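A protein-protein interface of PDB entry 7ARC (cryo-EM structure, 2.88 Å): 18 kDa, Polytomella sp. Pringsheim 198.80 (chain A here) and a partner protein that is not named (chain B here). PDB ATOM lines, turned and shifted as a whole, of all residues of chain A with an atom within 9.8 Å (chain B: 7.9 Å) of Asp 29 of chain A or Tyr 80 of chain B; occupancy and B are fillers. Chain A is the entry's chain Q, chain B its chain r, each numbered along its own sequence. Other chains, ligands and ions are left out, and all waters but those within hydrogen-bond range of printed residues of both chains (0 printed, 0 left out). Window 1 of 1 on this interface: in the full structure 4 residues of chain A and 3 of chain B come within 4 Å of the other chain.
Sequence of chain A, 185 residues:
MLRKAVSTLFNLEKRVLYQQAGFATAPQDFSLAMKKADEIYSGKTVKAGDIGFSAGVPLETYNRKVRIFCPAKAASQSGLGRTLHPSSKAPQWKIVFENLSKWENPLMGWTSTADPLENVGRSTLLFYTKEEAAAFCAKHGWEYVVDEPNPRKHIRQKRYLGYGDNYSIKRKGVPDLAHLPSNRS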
ATOM      1  N   THR A  25      -1.820 -12.059   6.812  1.00  0.00           N
ATOM      2  CA  THR A  25      -2.712 -11.461   7.797  1.00  0.00           C
ATOM      3  C   THR A  25      -2.713  -9.942   7.685  1.00  0.00           C
ATOM      4  O   THR A  25      -3.687  -9.349   7.210  1.00  0.00           O
ATOM      5  CB  THR A  25      -2.297 -11.876   9.209  1.00  0.00           C
ATOM      6  OG1 THR A  25      -0.946 -11.466   9.446  1.00  0.00           O
ATOM      7  CG2 THR A  25      -2.387 -13.383   9.363  1.00  0.00           C
ATOM      8  N   ALA A  26      -1.617  -9.311   8.108  1.00  0.00           N
ATOM      9  CA  ALA A  26      -1.437  -7.868   8.020  1.00  0.00           C
ATOM     10  C   ALA A  26       0.001  -7.507   8.368  1.00  0.00           C
ATOM     11  O   ALA A  26       0.595  -8.117   9.267  1.00  0.00           O
ATOM     12  CB  ALA A  26      -2.402  -7.133   8.952  1.00  0.00           C
ATOM     13  N   PRO A  27       0.596  -6.529   7.682  1.00  0.00           N
ATOM     14  CA  PRO A  27       1.911  -6.040   8.125  1.00  0.00           C
ATOM     15  C   PRO A  27       1.857  -5.317   9.460  1.00  0.00           C
ATOM     16  O   PRO A  27       2.776  -5.470  10.274  1.00  0.00           O
ATOM     17  CB  PRO A  27       2.344  -5.114   6.980  1.00  0.00           C
ATOM     18  CG  PRO A  27       1.071  -4.705   6.320  1.00  0.00           C
ATOM     19  CD  PRO A  27       0.146  -5.878   6.441  1.00  0.00           C
ATOM     20  N   GLN A  28       0.797  -4.542   9.709  1.00  0.00           N
ATOM     21  CA  GLN A  28       0.613  -3.803  10.962  1.00  0.00           C
ATOM     22  C   GLN A  28       1.810  -2.899  11.248  1.00  0.00           C
ATOM     23  O   GLN A  28       2.402  -2.923  12.328  1.00  0.00           O
ATOM     24  CB  GLN A  28       0.346  -4.751  12.134  1.00  0.00           C
ATOM     25  CG  GLN A  28      -0.972  -5.493  12.035  1.00  0.00           C
ATOM     26  CD  GLN A  28      -2.165  -4.595  12.296  1.00  0.00           C
ATOM     27  OE1 GLN A  28      -2.178  -3.825  13.255  1.00  0.00           O
ATOM     28  NE2 GLN A  28      -3.173  -4.686  11.437  1.00  0.00           N
ATOM     29  N   ASP A  29       2.158  -2.093  10.253  1.00  0.00           N
ATOM     30  CA  ASP A  29       3.256  -1.141  10.331  1.00  0.00           C
ATOM     31  C   ASP A  29       2.905   0.035   9.424  1.00  0.00           C
ATOM     32  O   ASP A  29       1.732   0.258   9.112  1.00  0.00           O
ATOM     33  CB  ASP A  29       4.587  -1.830   9.987  1.00  0.00           C
ATOM     34  CG  ASP A  29       4.621  -2.376   8.573  1.00  0.00           C
ATOM     35  OD1 ASP A  29       3.606  -2.269   7.858  1.00  0.00           O
ATOM     36  OD2 ASP A  29       5.672  -2.920   8.178  1.00  0.00           O
ATOM     37  N   PHE A  30       3.920   0.810   9.029  1.00  0.00           N
ATOM     38  CA  PHE A  30       3.701   1.957   8.151  1.00  0.00           C
ATOM     39  C   PHE A  30       2.892   1.593   6.909  1.00  0.00           C
ATOM     40  O   PHE A  30       2.168   2.439   6.367  1.00  0.00           O
ATOM     41  CB  PHE A  30       5.044   2.559   7.744  1.00  0.00           C
ATOM     42  CG  PHE A  30       4.964   4.000   7.345  1.00  0.00           C
ATOM     43  CD1 PHE A  30       4.331   4.922   8.158  1.00  0.00           C
ATOM     44  CD2 PHE A  30       5.518   4.435   6.154  1.00  0.00           C
ATOM     45  CE1 PHE A  30       4.256   6.248   7.793  1.00  0.00           C
ATOM     46  CE2 PHE A  30       5.446   5.759   5.786  1.00  0.00           C
ATOM     47  CZ  PHE A  30       4.814   6.667   6.605  1.00  0.00           C
ATOM     48  N   SER A  31       3.001   0.345   6.445  1.00  0.00           N
ATOM     49  CA  SER A  31       2.209  -0.099   5.303  1.00  0.00           C
ATOM     50  C   SER A  31       0.714   0.045   5.554  1.00  0.00           C
ATOM     51  O   SER A  31      -0.058   0.202   4.602  1.00  0.00           O
ATOM     52  CB  SER A  31       2.550  -1.550   4.962  1.00  0.00           C
ATOM     53  OG  SER A  31       2.125  -1.881   3.652  1.00  0.00           O
ATOM     54  N   LEU A  32       0.284   0.002   6.818  1.00  0.00           N
ATOM     55  CA  LEU A  32      -1.123   0.238   7.128  1.00  0.00           C
ATOM     56  C   LEU A  32      -1.552   1.628   6.678  1.00  0.00           C
ATOM     57  O   LEU A  32      -2.538   1.784   5.945  1.00  0.00           O
ATOM     58  CB  LEU A  32      -1.361   0.067   8.629  1.00  0.00           C
ATOM     59  CG  LEU A  32      -1.945  -1.255   9.126  1.00  0.00           C
ATOM     60  CD1 LEU A  32      -2.104  -1.213  10.632  1.00  0.00           C
ATOM     61  CD2 LEU A  32      -3.275  -1.540   8.454  1.00  0.00           C
ATOM     62  N   ALA A  33      -0.803   2.653   7.090  1.00  0.00           N
ATOM     63  CA  ALA A  33      -1.120   4.011   6.670  1.00  0.00           C
ATOM     64  C   ALA A  33      -0.906   4.197   5.177  1.00  0.00           C
ATOM     65  O   ALA A  33      -1.619   4.983   4.547  1.00  0.00           O
ATOM     66  CB  ALA A  33      -0.279   5.014   7.456  1.00  0.00           C
ATOM     67  N   MET A  34       0.050   3.474   4.591  1.00  0.00           N
ATOM     68  CA  MET A  34       0.252   3.545   3.146  1.00  0.00           C
ATOM     69  C   MET A  34      -0.992   3.076   2.396  1.00  0.00           C
ATOM     70  O   MET A  34      -1.518   3.782   1.526  1.00  0.00           O
ATOM     71  CB  MET A  34       1.470   2.710   2.755  1.00  0.00           C
ATOM     72  CG  MET A  34       2.786   3.239   3.303  1.00  0.00           C
ATOM     73  SD  MET A  34       3.206   4.896   2.735  1.00  0.00           S
ATOM     74  CE  MET A  34       3.557   4.578   1.009  1.00  0.00           C
ATOM     75  N   LYS A  35      -1.480   1.879   2.730  1.00  0.00           N
ATOM     76  CA  LYS A  35      -2.685   1.358   2.094  1.00  0.00           C
ATOM     77  C   LYS A  35      -3.893   2.242   2.378  1.00  0.00           C
ATOM     78  O   LYS A  35      -4.773   2.400   1.522  1.00  0.00           O
ATOM     79  CB  LYS A  35      -2.957  -0.068   2.574  1.00  0.00           C
ATOM     80  CG  LYS A  35      -1.866  -1.105   2.288  1.00  0.00           C
ATOM     81  CD  LYS A  35      -1.741  -1.477   0.814  1.00  0.00           C
ATOM     82  CE  LYS A  35      -0.686  -0.646   0.098  1.00  0.00           C
ATOM     83  NZ  LYS A  35      -0.497  -1.089  -1.310  1.00  0.00           N
ATOM     84  N   LYS A  36      -3.965   2.815   3.583  1.00  0.00           N
ATOM     85  CA  LYS A  36      -5.132   3.621   3.922  1.00  0.00           C
ATOM     86  C   LYS A  36      -5.134   4.917   3.115  1.00  0.00           C
ATOM     87  O   LYS A  36      -6.183   5.356   2.626  1.00  0.00           O
ATOM     88  CB  LYS A  36      -5.133   3.899   5.425  1.00  0.00           C
ATOM     89  CG  LYS A  36      -6.313   4.687   5.962  1.00  0.00           C
ATOM     90  CD  LYS A  36      -7.565   3.822   5.823  1.00  0.00           C
ATOM     91  CE  LYS A  36      -8.814   4.460   6.402  1.00  0.00           C
ATOM     92  NZ  LYS A  36      -9.262   5.670   5.686  1.00  0.00           N
ATOM     93  N   LYS A  89       5.204  -8.759   0.908  1.00  0.00           N
ATOM     94  CA  LYS A  89       4.448  -7.516   1.026  1.00  0.00           C
ATOM     95  C   LYS A  89       5.021  -6.399   0.163  1.00  0.00           C
ATOM     96  O   LYS A  89       4.574  -5.253   0.279  1.00  0.00           O
ATOM     97  CB  LYS A  89       4.371  -7.022   2.475  1.00  0.00           C
ATOM     98  CG  LYS A  89       3.299  -7.653   3.356  1.00  0.00           C
ATOM     99  CD  LYS A  89       3.638  -9.059   3.771  1.00  0.00           C
ATOM    100  CE  LYS A  89       4.808  -9.046   4.746  1.00  0.00           C
ATOM    101  NZ  LYS A  89       5.145 -10.410   5.236  1.00  0.00           N
ATOM    102  N   ALA A  90       5.991  -6.693  -0.697  1.00  0.00           N
ATOM    103  CA  ALA A  90       6.607  -5.654  -1.506  1.00  0.00           C
ATOM    104  C   ALA A  90       6.095  -5.697  -2.937  1.00  0.00           C
ATOM    105  O   ALA A  90       5.625  -6.735  -3.412  1.00  0.00           O
ATOM    106  CB  ALA A  90       8.130  -5.813  -1.499  1.00  0.00           C
ATOM    107  N   TYR A 128       2.418  -3.215  -7.136  1.00  0.00           N
ATOM    108  CA  TYR A 128       1.820  -4.263  -6.317  1.00  0.00           C
ATOM    109  C   TYR A 128       1.003  -5.236  -7.154  1.00  0.00           C
ATOM    110  O   TYR A 128       1.002  -6.443  -6.886  1.00  0.00           O
ATOM    111  CB  TYR A 128       0.945  -3.642  -5.231  1.00  0.00           C
ATOM    112  CG  TYR A 128       1.713  -3.162  -4.029  1.00  0.00           C
ATOM    113  CD1 TYR A 128       1.846  -1.809  -3.760  1.00  0.00           C
ATOM    114  CD2 TYR A 128       2.312  -4.064  -3.165  1.00  0.00           C
ATOM    115  CE1 TYR A 128       2.552  -1.366  -2.662  1.00  0.00           C
ATOM    116  CE2 TYR A 128       3.019  -3.633  -2.064  1.00  0.00           C
ATOM    117  CZ  TYR A 128       3.137  -2.284  -1.817  1.00  0.00           C
ATOM    118  OH  TYR A 128       3.841  -1.851  -0.718  1.00  0.00           O
ATOM    119  N   ASN B  77      10.970  -4.745  15.658  1.00  0.00           N
ATOM    120  CA  ASN B  77       9.944  -4.908  16.682  1.00  0.00           C
ATOM    121  C   ASN B  77       9.046  -3.682  16.829  1.00  0.00           C
ATOM    122  O   ASN B  77       8.365  -3.540  17.850  1.00  0.00           O
ATOM    123  CB  ASN B  77      10.595  -5.252  18.021  1.00  0.00           C
ATOM    124  CG  ASN B  77      10.821  -6.739  18.190  1.00  0.00           C
ATOM    125  OD1 ASN B  77      10.042  -7.556  17.701  1.00  0.00           O
ATOM    126  ND2 ASN B  77      11.895  -7.098  18.883  1.00  0.00           N
ATOM    127  N   ASN B  78       9.030  -2.795  15.840  1.00  0.00           N
ATOM    128  CA  ASN B  78       8.149  -1.635  15.850  1.00  0.00           C
ATOM    129  C   ASN B  78       6.831  -1.958  15.154  1.00  0.00           C
ATOM    130  O   ASN B  78       6.791  -2.724  14.189  1.00  0.00           O
ATOM    131  CB  ASN B  78       8.818  -0.439  15.174  1.00  0.00           C
ATOM    132  CG  ASN B  78      10.057   0.024  15.907  1.00  0.00           C
ATOM    133  OD1 ASN B  78       9.981   0.497  17.039  1.00  0.00           O
ATOM    134  ND2 ASN B  78      11.209  -0.110  15.263  1.00  0.00           N
ATOM    135  N   SER B  79       5.747  -1.367  15.656  1.00  0.00           N
ATOM    136  CA  SER B  79       4.425  -1.592  15.087  1.00  0.00           C
ATOM    137  C   SER B  79       3.606  -0.309  15.153  1.00  0.00           C
ATOM    138  O   SER B  79       3.958   0.648  15.847  1.00  0.00           O
ATOM    139  CB  SER B  79       3.694  -2.729  15.810  1.00  0.00           C
ATOM    140  OG  SER B  79       2.397  -2.924  15.275  1.00  0.00           O
ATOM    141  N   TYR B  80       2.500  -0.301  14.410  1.00  0.00           N
ATOM    142  CA  TYR B  80       1.596   0.840  14.325  1.00  0.00           C
ATOM    143  C   TYR B  80       0.195   0.410  14.738  1.00  0.00           C
ATOM    144  O   TYR B  80      -0.373  -0.510  14.141  1.00  0.00           O
ATOM    145  CB  TYR B  80       1.579   1.410  12.907  1.00  0.00           C
ATOM    146  CG  TYR B  80       2.463   2.619  12.719  1.00  0.00           C
ATOM    147  CD1 TYR B  80       3.817   2.474  12.458  1.00  0.00           C
ATOM    148  CD2 TYR B  80       1.945   3.901  12.807  1.00  0.00           C
ATOM    149  CE1 TYR B  80       4.629   3.573  12.285  1.00  0.00           C
ATOM    150  CE2 TYR B  80       2.751   5.005  12.638  1.00  0.00           C
ATOM    151  CZ  TYR B  80       4.091   4.835  12.377  1.00  0.00           C
ATOM    152  OH  TYR B  80       4.898   5.933  12.206  1.00  0.00           O
ATOM    153  N   THR B  81      -0.360   1.070  15.749  1.00  0.00           N
ATOM    154  CA  THR B  81      -1.743   0.831  16.135  1.00  0.00           C
ATOM    155  C   THR B  81      -2.673   1.803  15.407  1.00  0.00           C
ATOM    156  O   THR B  81      -2.238   2.750  14.751  1.00  0.00           O
ATOM    157  CB  THR B  81      -1.913   0.946  17.650  1.00  0.00           C
ATOM    158  OG1 THR B  81      -3.192   0.422  18.028  1.00  0.00           O
ATOM    159  CG2 THR B  81      -1.820   2.389  18.094  1.00  0.00           C
ATOM    160  N   VAL B  82      -3.976   1.550  15.523  1.00  0.00           N
ATOM    161  CA  VAL B  82      -4.994   2.282  14.778  1.00  0.00           C
ATOM    162  C   VAL B  82      -6.049   2.807  15.743  1.00  0.00           C
ATOM    163  O   VAL B  82      -6.489   2.088  16.646  1.00  0.00           O
ATOM    164  CB  VAL B  82      -5.650   1.395  13.697  1.00  0.00           C
ATOM    165  CG1 VAL B  82      -6.776   2.139  12.998  1.00  0.00           C
ATOM    166  CG2 VAL B  82      -4.616   0.922  12.694  1.00  0.00           C
ATOM    167  N   ARG B  83      -6.454   4.062  15.552  1.00  0.00           N
ATOM    168  CA  ARG B  83      -7.589   4.631  16.262  1.00  0.00           C
ATOM    169  C   ARG B  83      -8.470   5.393  15.281  1.00  0.00           C
ATOM    170  O   ARG B  83      -8.047   5.755  14.181  1.00  0.00           O
ATOM    171  CB  ARG B  83      -7.167   5.584  17.390  1.00  0.00           C
ATOM    172  CG  ARG B  83      -6.478   4.923  18.560  1.00  0.00           C
ATOM    173  CD  ARG B  83      -6.184   5.937  19.652  1.00  0.00           C
ATOM    174  NE  ARG B  83      -5.166   6.908  19.273  1.00  0.00           N
ATOM    175  CZ  ARG B  83      -5.399   8.201  19.091  1.00  0.00           C
ATOM    176  NH1 ARG B  83      -6.616   8.706  19.210  1.00  0.00           N
ATOM    177  NH2 ARG B  83      -4.387   9.006  18.785  1.00  0.00           N
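Of the 15 printed residues of chain A, 4 touch a printed residue of chain B.
Hydrophobic or aromatic side chains of chain A that line the printed part of chain B: Leu 32.
Of the 7 printed residues of chain B, 3 touch a printed residue of chain A.
Along chain B the printed residues that touch a printed residue of chain A span positions 79 to 82.
Among the printed residues, pairs that only touch across the chains: Phe 30 of chain A with Tyr 80 of chain B, Leu 32 of chain A with Val 82 of chain B, Asp 29 of chain A with Tyr 80 of chain B and Leu 32 of chain A with Tyr 80 of chain B.
N of Tyr 80 of chain B lies within hydrogen-bond range of O of Gln 28 of chain A (3.3 Å).
The side-chain hydroxyl of Ser 79 of chain B sits at hydrogen-bond distance from the backbone carbonyl oxygen of Gln 28 of chain A, 2.9 Å away.
The backbone NH (N) of Ser 31 of chain A lies close to the side-chain carboxylate (OD1) of Asp 29 of chain A (3.0 Å).
Of the printed residues of chain B, Gln 28 of chain A touches Ser 79 and Tyr 80.
Asp 29 of chain A touches one residue of chain B.
Of the printed residues of chain B, Phe 30 of chain A touches Tyr 80.
Printed residues of chain B within 4 Å of Leu 32 of chain A: Tyr 80 and Val 82.
Tyr 80 of chain B touches just these residues of chain A: Gln 28, Asp 29, Phe 30 and Leu 32.
Printed residues of chain A within 4 Å of Val 82 of chain B: Leu 32.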
